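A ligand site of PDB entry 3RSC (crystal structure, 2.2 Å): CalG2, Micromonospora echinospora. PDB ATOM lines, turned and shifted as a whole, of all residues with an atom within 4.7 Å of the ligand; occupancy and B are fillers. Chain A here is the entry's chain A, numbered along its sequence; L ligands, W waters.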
ATOM      1  N   LEU A  33       6.705  15.427 -16.705  1.00  0.00           N
ATOM      2  CA  LEU A  33       7.200  16.553 -15.922  1.00  0.00           C
ATOM      3  C   LEU A  33       7.255  16.246 -14.421  1.00  0.00           C
ATOM      4  O   LEU A  33       8.116  16.759 -13.707  1.00  0.00           O
ATOM      5  CB  LEU A  33       6.318  17.788 -16.158  1.00  0.00           C
ATOM      6  CG  LEU A  33       6.729  18.733 -17.297  1.00  0.00           C
ATOM      7  CD1 LEU A  33       7.287  17.991 -18.504  1.00  0.00           C
ATOM      8  CD2 LEU A  33       5.570  19.643 -17.695  1.00  0.00           C
ATOM      9  N   ILE A  77      -4.645  21.267 -19.242  1.00  0.00           N
ATOM     10  CA  ILE A  77      -3.868  20.344 -20.064  1.00  0.00           C
ATOM     11  C   ILE A  77      -4.111  18.896 -19.666  1.00  0.00           C
ATOM     12  O   ILE A  77      -4.084  17.996 -20.502  1.00  0.00           O
ATOM     13  CB  ILE A  77      -2.354  20.670 -20.056  1.00  0.00           C
ATOM     14  CG1 ILE A  77      -1.744  20.419 -18.673  1.00  0.00           C
ATOM     15  CG2 ILE A  77      -2.120  22.110 -20.503  1.00  0.00           C
ATOM     16  CD1 ILE A  77      -0.233  20.610 -18.633  1.00  0.00           C
ATOM     17  N   ALA A  82      -3.366  16.600 -26.893  1.00  0.00           N
ATOM     18  CA  ALA A  82      -2.359  17.473 -27.501  1.00  0.00           C
ATOM     19  C   ALA A  82      -2.420  17.454 -29.019  1.00  0.00           C
ATOM     20  O   ALA A  82      -2.267  18.486 -29.669  1.00  0.00           O
ATOM     21  CB  ALA A  82      -0.972  17.091 -27.028  1.00  0.00           C
ATOM     22  N   VAL A  85      -5.273  19.718 -29.792  1.00  0.00           N
ATOM     23  CA  VAL A  85      -4.955  21.116 -29.516  1.00  0.00           C
ATOM     24  C   VAL A  85      -4.077  21.714 -30.609  1.00  0.00           C
ATOM     25  O   VAL A  85      -4.378  22.780 -31.142  1.00  0.00           O
ATOM     26  CB  VAL A  85      -4.278  21.286 -28.144  1.00  0.00           C
ATOM     27  CG1 VAL A  85      -3.782  22.723 -27.977  1.00  0.00           C
ATOM     28  CG2 VAL A  85      -5.241  20.927 -27.025  1.00  0.00           C
ATOM     29  N   PHE A  86      -2.982  21.026 -30.931  1.00  0.00           N
ATOM     30  CA  PHE A  86      -2.056  21.496 -31.951  1.00  0.00           C
ATOM     31  C   PHE A  86      -2.604  21.338 -33.373  1.00  0.00           C
ATOM     32  O   PHE A  86      -2.070  21.914 -34.330  1.00  0.00           O
ATOM     33  CB  PHE A  86      -0.685  20.813 -31.804  1.00  0.00           C
ATOM     34  CG  PHE A  86       0.165  21.392 -30.707  1.00  0.00           C
ATOM     35  CD1 PHE A  86       0.969  22.509 -30.945  1.00  0.00           C
ATOM     36  CD2 PHE A  86       0.156  20.848 -29.440  1.00  0.00           C
ATOM     37  CE1 PHE A  86       1.742  23.052 -29.933  1.00  0.00           C
ATOM     38  CE2 PHE A  86       0.933  21.397 -28.422  1.00  0.00           C
ATOM     39  CZ  PHE A  86       1.728  22.501 -28.672  1.00  0.00           C
ATOM     40  N   PRO A  95      -3.023  26.347 -28.731  1.00  0.00           N
ATOM     41  CA  PRO A  95      -2.010  25.918 -27.759  1.00  0.00           C
ATOM     42  C   PRO A  95      -1.354  27.102 -27.046  1.00  0.00           C
ATOM     43  O   PRO A  95      -1.271  27.096 -25.818  1.00  0.00           O
ATOM     44  CB  PRO A  95      -0.986  25.153 -28.606  1.00  0.00           C
ATOM     45  CG  PRO A  95      -1.265  25.534 -30.023  1.00  0.00           C
ATOM     46  CD  PRO A  95      -2.740  25.837 -30.084  1.00  0.00           C
ATOM     47  N   HIS A  96      -0.917  28.108 -27.805  1.00  0.00           N
ATOM     48  CA  HIS A  96      -0.285  29.282 -27.194  1.00  0.00           C
ATOM     49  C   HIS A  96      -1.110  29.862 -26.056  1.00  0.00           C
ATOM     50  O   HIS A  96      -0.593  30.109 -24.965  1.00  0.00           O
ATOM     51  CB  HIS A  96      -0.003  30.370 -28.240  1.00  0.00           C
ATOM     52  CG  HIS A  96       1.060  30.007 -29.220  1.00  0.00           C
ATOM     53  ND1 HIS A  96       1.814  28.847 -29.124  1.00  0.00           N
ATOM     54  CD2 HIS A  96       1.498  30.628 -30.337  1.00  0.00           C
ATOM     55  CE1 HIS A  96       2.664  28.791 -30.129  1.00  0.00           C
ATOM     56  NE2 HIS A  96       2.501  29.862 -30.883  1.00  0.00           N
ATOM     57  N   MET A  98      -3.673  28.464 -24.438  1.00  0.00           N
ATOM     58  CA  MET A  98      -3.889  27.490 -23.379  1.00  0.00           C
ATOM     59  C   MET A  98      -2.663  27.473 -22.454  1.00  0.00           C
ATOM     60  O   MET A  98      -2.796  27.448 -21.225  1.00  0.00           O
ATOM     61  CB  MET A  98      -4.157  26.097 -23.948  1.00  0.00           C
ATOM     62  CG  MET A  98      -4.458  25.057 -22.876  1.00  0.00           C
ATOM     63  SD  MET A  98      -4.846  23.279 -23.582  1.00  0.00           S
ATOM     64  CE  MET A  98      -6.537  23.671 -24.472  1.00  0.00           C
ATOM     65  N   TYR A  99      -1.486  27.490 -23.065  1.00  0.00           N
ATOM     66  CA  TYR A  99      -0.230  27.566 -22.322  1.00  0.00           C
ATOM     67  C   TYR A  99      -0.243  28.721 -21.318  1.00  0.00           C
ATOM     68  O   TYR A  99       0.133  28.553 -20.157  1.00  0.00           O
ATOM     69  CB  TYR A  99       0.932  27.733 -23.287  1.00  0.00           C
ATOM     70  CG  TYR A  99       2.294  27.848 -22.623  1.00  0.00           C
ATOM     71  CD1 TYR A  99       2.958  26.718 -22.164  1.00  0.00           C
ATOM     72  CD2 TYR A  99       2.895  29.080 -22.451  1.00  0.00           C
ATOM     73  CE1 TYR A  99       4.201  26.816 -21.564  1.00  0.00           C
ATOM     74  CE2 TYR A  99       4.127  29.197 -21.848  1.00  0.00           C
ATOM     75  CZ  TYR A  99       4.776  28.060 -21.404  1.00  0.00           C
ATOM     76  OH  TYR A  99       6.006  28.161 -20.798  1.00  0.00           O
ATOM     77  N   ASP A 126      10.099  23.783 -16.478  1.00  0.00           N
ATOM     78  CA  ASP A 126      10.176  24.616 -17.680  1.00  0.00           C
ATOM     79  C   ASP A 126       8.811  25.167 -18.090  1.00  0.00           C
ATOM     80  O   ASP A 126       8.666  26.365 -18.369  1.00  0.00           O
ATOM     81  CB  ASP A 126      10.762  23.835 -18.862  1.00  0.00           C
ATOM     82  CG  ASP A 126      12.198  23.378 -18.631  1.00  0.00           C
ATOM     83  OD1 ASP A 126      13.017  24.152 -18.101  1.00  0.00           O
ATOM     84  OD2 ASP A 126      12.501  22.226 -19.013  1.00  0.00           O
ATOM     85  N   PHE A 127       7.811  24.292 -18.124  1.00  0.00           N
ATOM     86  CA  PHE A 127       6.475  24.646 -18.631  1.00  0.00           C
ATOM     87  C   PHE A 127       5.865  25.864 -17.910  1.00  0.00           C
ATOM     88  O   PHE A 127       5.502  26.838 -18.561  1.00  0.00           O
ATOM     89  CB  PHE A 127       5.538  23.421 -18.607  1.00  0.00           C
ATOM     90  CG  PHE A 127       4.202  23.651 -19.270  1.00  0.00           C
ATOM     91  CD1 PHE A 127       3.314  24.583 -18.784  1.00  0.00           C
ATOM     92  CD2 PHE A 127       3.829  22.907 -20.378  1.00  0.00           C
ATOM     93  CE1 PHE A 127       2.078  24.790 -19.392  1.00  0.00           C
ATOM     94  CE2 PHE A 127       2.603  23.095 -20.988  1.00  0.00           C
ATOM     95  CZ  PHE A 127       1.728  24.044 -20.497  1.00  0.00           C
ATOM     96  N   SER A 159      12.774  25.497 -26.397  1.00  0.00           N
ATOM     97  CA  SER A 159      11.528  26.137 -26.772  1.00  0.00           C
ATOM     98  C   SER A 159      11.474  26.464 -28.262  1.00  0.00           C
ATOM     99  O   SER A 159      10.535  26.069 -28.954  1.00  0.00           O
ATOM    100  CB  SER A 159      11.306  27.413 -25.967  1.00  0.00           C
ATOM    101  OG  SER A 159      11.058  27.118 -24.600  1.00  0.00           O
ATOM    102  N   MET A 162      11.217  23.404 -30.409  1.00  0.00           N
ATOM    103  CA  MET A 162       9.861  22.880 -30.437  1.00  0.00           C
ATOM    104  C   MET A 162       8.887  23.748 -31.246  1.00  0.00           C
ATOM    105  O   MET A 162       8.045  23.206 -31.974  1.00  0.00           O
ATOM    106  CB  MET A 162       9.343  22.659 -29.020  1.00  0.00           C
ATOM    107  CG  MET A 162       9.917  21.392 -28.391  1.00  0.00           C
ATOM    108  SD  MET A 162       8.844  20.760 -26.895  1.00  0.00           S
ATOM    109  CE  MET A 162       9.018  22.284 -25.702  1.00  0.00           C
ATOM    110  N   VAL A 163       8.998  25.062 -31.129  1.00  0.00           N
ATOM    111  CA  VAL A 163       8.184  25.956 -31.959  1.00  0.00           C
ATOM    112  C   VAL A 163       8.373  25.628 -33.441  1.00  0.00           C
ATOM    113  O   VAL A 163       7.423  25.299 -34.132  1.00  0.00           O
ATOM    114  CB  VAL A 163       8.516  27.444 -31.706  1.00  0.00           C
ATOM    115  CG1 VAL A 163       7.882  28.319 -32.793  1.00  0.00           C
ATOM    116  CG2 VAL A 163       8.049  27.872 -30.324  1.00  0.00           C
ATOM    117  N   ALA A 166       7.148  22.226 -34.436  1.00  0.00           N
ATOM    118  CA  ALA A 166       5.687  22.127 -34.367  1.00  0.00           C
ATOM    119  C   ALA A 166       5.016  22.895 -35.507  1.00  0.00           C
ATOM    120  O   ALA A 166       3.874  22.605 -35.875  1.00  0.00           O
ATOM    121  CB  ALA A 166       5.188  22.618 -33.013  1.00  0.00           C
ATOM    122  N   THR A 168       4.258  26.070 -35.530  1.00  0.00           N
ATOM    123  CA  THR A 168       3.385  27.130 -35.046  1.00  0.00           C
ATOM    124  C   THR A 168       4.066  28.487 -35.202  1.00  0.00           C
ATOM    125  O   THR A 168       5.270  28.579 -35.398  1.00  0.00           O
ATOM    126  CB  THR A 168       3.025  26.958 -33.560  1.00  0.00           C
ATOM    127  OG1 THR A 168       4.173  27.242 -32.743  1.00  0.00           O
ATOM    128  CG2 THR A 168       2.553  25.536 -33.280  1.00  0.00           C
ATOM    129  N   PRO A 171       5.286  32.389 -30.411  1.00  0.00           N
ATOM    130  CA  PRO A 171       4.296  32.963 -29.496  1.00  0.00           C
ATOM    131  C   PRO A 171       4.428  34.478 -29.365  1.00  0.00           C
ATOM    132  O   PRO A 171       3.420  35.172 -29.218  1.00  0.00           O
ATOM    133  CB  PRO A 171       4.635  32.281 -28.167  1.00  0.00           C
ATOM    134  CG  PRO A 171       5.223  30.971 -28.568  1.00  0.00           C
ATOM    135  CD  PRO A 171       6.002  31.249 -29.816  1.00  0.00           C
ATOM    136  N   TRP A 198      10.793  36.018 -21.238  1.00  0.00           N
ATOM    137  CA  TRP A 198      10.632  34.814 -22.030  1.00  0.00           C
ATOM    138  C   TRP A 198      11.935  34.035 -22.152  1.00  0.00           C
ATOM    139  O   TRP A 198      11.942  32.807 -22.182  1.00  0.00           O
ATOM    140  CB  TRP A 198      10.108  35.151 -23.415  1.00  0.00           C
ATOM    141  CG  TRP A 198       9.687  33.937 -24.154  1.00  0.00           C
ATOM    142  CD1 TRP A 198      10.428  33.208 -25.030  1.00  0.00           C
ATOM    143  CD2 TRP A 198       8.418  33.286 -24.057  1.00  0.00           C
ATOM    144  NE1 TRP A 198       9.697  32.149 -25.491  1.00  0.00           N
ATOM    145  CE2 TRP A 198       8.458  32.173 -24.916  1.00  0.00           C
ATOM    146  CE3 TRP A 198       7.252  33.547 -23.334  1.00  0.00           C
ATOM    147  CZ2 TRP A 198       7.376  31.308 -25.066  1.00  0.00           C
ATOM    148  CZ3 TRP A 198       6.175  32.687 -23.492  1.00  0.00           C
ATOM    149  CH2 TRP A 198       6.248  31.582 -24.350  1.00  0.00           C
ATOM    150  N   THR A 257       1.387  11.034 -24.603  1.00  0.00           N
ATOM    151  CA  THR A 257       0.974  12.295 -25.204  1.00  0.00           C
ATOM    152  C   THR A 257       0.392  12.178 -26.615  1.00  0.00           C
ATOM    153  O   THR A 257      -0.746  12.608 -26.853  1.00  0.00           O
ATOM    154  CB  THR A 257       2.121  13.342 -25.177  1.00  0.00           C
ATOM    155  OG1 THR A 257       2.694  13.389 -23.862  1.00  0.00           O
ATOM    156  CG2 THR A 257       1.606  14.720 -25.549  1.00  0.00           C
ATOM    157  N   PHE A 258       1.164  11.640 -27.555  1.00  0.00           N
ATOM    158  CA  PHE A 258       0.689  11.427 -28.917  1.00  0.00           C
ATOM    159  C   PHE A 258       0.506   9.947 -29.209  1.00  0.00           C
ATOM    160  O   PHE A 258       1.114   9.395 -30.124  1.00  0.00           O
ATOM    161  CB  PHE A 258       1.663  12.034 -29.938  1.00  0.00           C
ATOM    162  CG  PHE A 258       1.744  13.527 -29.895  1.00  0.00           C
ATOM    163  CD1 PHE A 258       2.653  14.164 -29.057  1.00  0.00           C
ATOM    164  CD2 PHE A 258       0.930  14.303 -30.695  1.00  0.00           C
ATOM    165  CE1 PHE A 258       2.733  15.544 -29.020  1.00  0.00           C
ATOM    166  CE2 PHE A 258       0.998  15.682 -30.666  1.00  0.00           C
ATOM    167  CZ  PHE A 258       1.905  16.302 -29.825  1.00  0.00           C
ATOM    168  N   PHE A 343       6.415  16.430 -32.806  1.00  0.00           N
ATOM    169  CA  PHE A 343       7.456  17.443 -32.737  1.00  0.00           C
ATOM    170  C   PHE A 343       8.212  17.473 -31.411  1.00  0.00           C
ATOM    171  O   PHE A 343       9.400  17.787 -31.370  1.00  0.00           O
ATOM    172  CB  PHE A 343       6.859  18.830 -33.016  1.00  0.00           C
ATOM    173  CG  PHE A 343       6.020  19.345 -31.882  1.00  0.00           C
ATOM    174  CD1 PHE A 343       4.639  19.176 -31.888  1.00  0.00           C
ATOM    175  CD2 PHE A 343       6.610  19.991 -30.797  1.00  0.00           C
ATOM    176  CE1 PHE A 343       3.870  19.639 -30.839  1.00  0.00           C
ATOM    177  CE2 PHE A 343       5.841  20.454 -29.748  1.00  0.00           C
ATOM    178  CZ  PHE A 343       4.470  20.293 -29.769  1.00  0.00           C
ATOM    179  N   ASP A 344       7.516  17.169 -30.318  1.00  0.00           N
ATOM    180  CA  ASP A 344       8.056  17.343 -28.972  1.00  0.00           C
ATOM    181  C   ASP A 344       9.228  16.411 -28.655  1.00  0.00           C
ATOM    182  O   ASP A 344      10.000  16.687 -27.744  1.00  0.00           O
ATOM    183  CB  ASP A 344       6.956  17.180 -27.923  1.00  0.00           C
ATOM    184  CG  ASP A 344       6.265  15.822 -27.998  1.00  0.00           C
ATOM    185  OD1 ASP A 344       6.150  15.257 -29.112  1.00  0.00           O
ATOM    186  OD2 ASP A 344       5.828  15.324 -26.947  1.00  0.00           O
HETATM  187  C1  LIG L   1       5.006  27.463 -25.308  1.00  0.00           C
HETATM  188  N1  LIG L   1       6.601  25.839 -24.536  1.00  0.00           N
HETATM  189  O1  LIG L   1       5.560  28.356 -24.700  1.00  0.00           O
HETATM  190  S1  LIG L   1       0.523  23.747 -23.591  1.00  0.00           S
HETATM  191  C2  LIG L   1       5.415  26.076 -25.081  1.00  0.00           C
HETATM  192  N2  LIG L   1       5.529  17.470 -24.604  1.00  0.00           N
HETATM  193  O2  LIG L   1       5.845  24.461 -22.936  1.00  0.00           O
HETATM  194  S2  LIG L   1      -1.040  23.483 -24.828  1.00  0.00           S
HETATM  195  C3  LIG L   1       4.615  25.089 -25.445  1.00  0.00           C
HETATM  196  O3  LIG L   1       8.100  24.852 -22.955  1.00  0.00           O
HETATM  197  S3  LIG L   1      -1.764  21.630 -24.629  1.00  0.00           S
HETATM  198  C4  LIG L   1       3.238  25.398 -25.831  1.00  0.00           C
HETATM  199  O4  LIG L   1       1.767  26.900 -26.939  1.00  0.00           O
HETATM  200  C5  LIG L   1       3.148  26.559 -26.792  1.00  0.00           C
HETATM  201  O5  LIG L   1       4.136  22.718 -25.098  1.00  0.00           O
HETATM  202  C6  LIG L   1       3.906  27.787 -26.289  1.00  0.00           C
HETATM  203  O6  LIG L   1       5.033  16.356 -24.905  1.00  0.00           O
HETATM  204  C7  LIG L   1       6.764  25.043 -23.481  1.00  0.00           C
HETATM  205  O7  LIG L   1       3.814  20.477 -25.660  1.00  0.00           O
HETATM  206  C8  LIG L   1       8.404  23.736 -22.116  1.00  0.00           C
HETATM  207  O8  LIG L   1       5.936  21.894 -23.041  1.00  0.00           O
HETATM  208  C9  LIG L   1       3.656  26.123 -28.098  1.00  0.00           C
HETATM  209  O9  LIG L   1       5.527  19.137 -22.188  1.00  0.00           O
HETATM  210  C10 LIG L   1       4.166  25.634 -29.046  1.00  0.00           C
HETATM  211  C11 LIG L   1       4.904  24.829 -29.952  1.00  0.00           C
HETATM  212  C12 LIG L   1       5.605  23.788 -29.500  1.00  0.00           C
HETATM  213  C13 LIG L   1       5.617  23.497 -28.099  1.00  0.00           C
HETATM  214  C14 LIG L   1       5.459  23.487 -26.933  1.00  0.00           C
HETATM  215  C15 LIG L   1       5.112  23.672 -25.515  1.00  0.00           C
HETATM  216  C16 LIG L   1       2.103  24.798 -25.445  1.00  0.00           C
HETATM  217  C17 LIG L   1       2.033  23.636 -24.490  1.00  0.00           C
HETATM  218  C18 LIG L   1      -0.999  20.560 -25.800  1.00  0.00           C
HETATM  219  C19 LIG L   1       4.702  21.414 -25.062  1.00  0.00           C
HETATM  220  C20 LIG L   1       4.980  21.008 -23.618  1.00  0.00           C
HETATM  221  C21 LIG L   1       5.524  19.578 -23.544  1.00  0.00           C
HETATM  222  C22 LIG L   1       4.677  18.623 -24.374  1.00  0.00           C
HETATM  223  C23 LIG L   1       4.404  19.191 -25.769  1.00  0.00           C
HETATM  224  C24 LIG L   1       3.474  18.275 -26.555  1.00  0.00           C
HETATM  225  O   HOH W   1       3.790  15.304 -22.360  1.00  0.00           O
HETATM  226  O   HOH W   2      10.773  21.687 -21.510  1.00  0.00           O
HETATM  227  O   HOH W   3       7.477  14.394 -24.361  1.00  0.00           O
HETATM  228  O   HOH W   4       4.831  17.266 -20.633  1.00  0.00           O
HETATM  229  O   HOH W   5       8.673  18.751 -23.098  1.00  0.00           O
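The side-chain sulfur (SD) of Met 98 lies close to a sulfur (S3) of the ligand (3.6 Å). Ala 82 touches the ligand (CB to C18, 3.7 Å). Phe 86 touches the ligand (CE2 to C18, 3.4 Å). Tyr 99 touches the ligand. Phe 127 touches the ligand. Met 162 touches the ligand. Val 163 touches the ligand. CB of Ala 166 touches C12 of the ligand, at 3.7 Å. OG1 of Thr 168 touches C11 of the ligand, at 3.8 Å. CH2 of Trp 198 touches O1 of the ligand, 3.3 Å away. Thr 257 touches the ligand. Phe 258 touches the ligand (CE1 to C24, 3.8 Å). Phe 343 touches the ligand. Of the 22 residues printed, 16 come within 4 Å of the ligand.
The backbone carbonyl oxygen (O) of Pro 95 lies close to an oxygen (O4) of the ligand (3.2 Å). OD2 of Asp 344 lies within hydrogen-bond range of O6 of the ligand, at 2.4 Å. An oxygen (O4) of the ligand is in hydrogen-bond range of the backbone NH (N) of His 96, at 3.1 Å. A ring nitrogen (ND1) of His 96 is in hydrogen-bond range of an oxygen (O4) of the ligand, 2.9 Å away.
Water W1 bridges the side-chain hydroxyl of Thr 257 and an oxygen (O6) of the ligand. Water W3 lies within hydrogen-bond range of an oxygen (O6) of the ligand (3.2 Å) and the side-chain carboxylate of Asp 344 (3.2 Å).
The side-chain hydroxyl (OH) of Tyr 99 is in hydrogen-bond range of the backbone carbonyl oxygen (O) of Phe 127 (2.6 Å).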
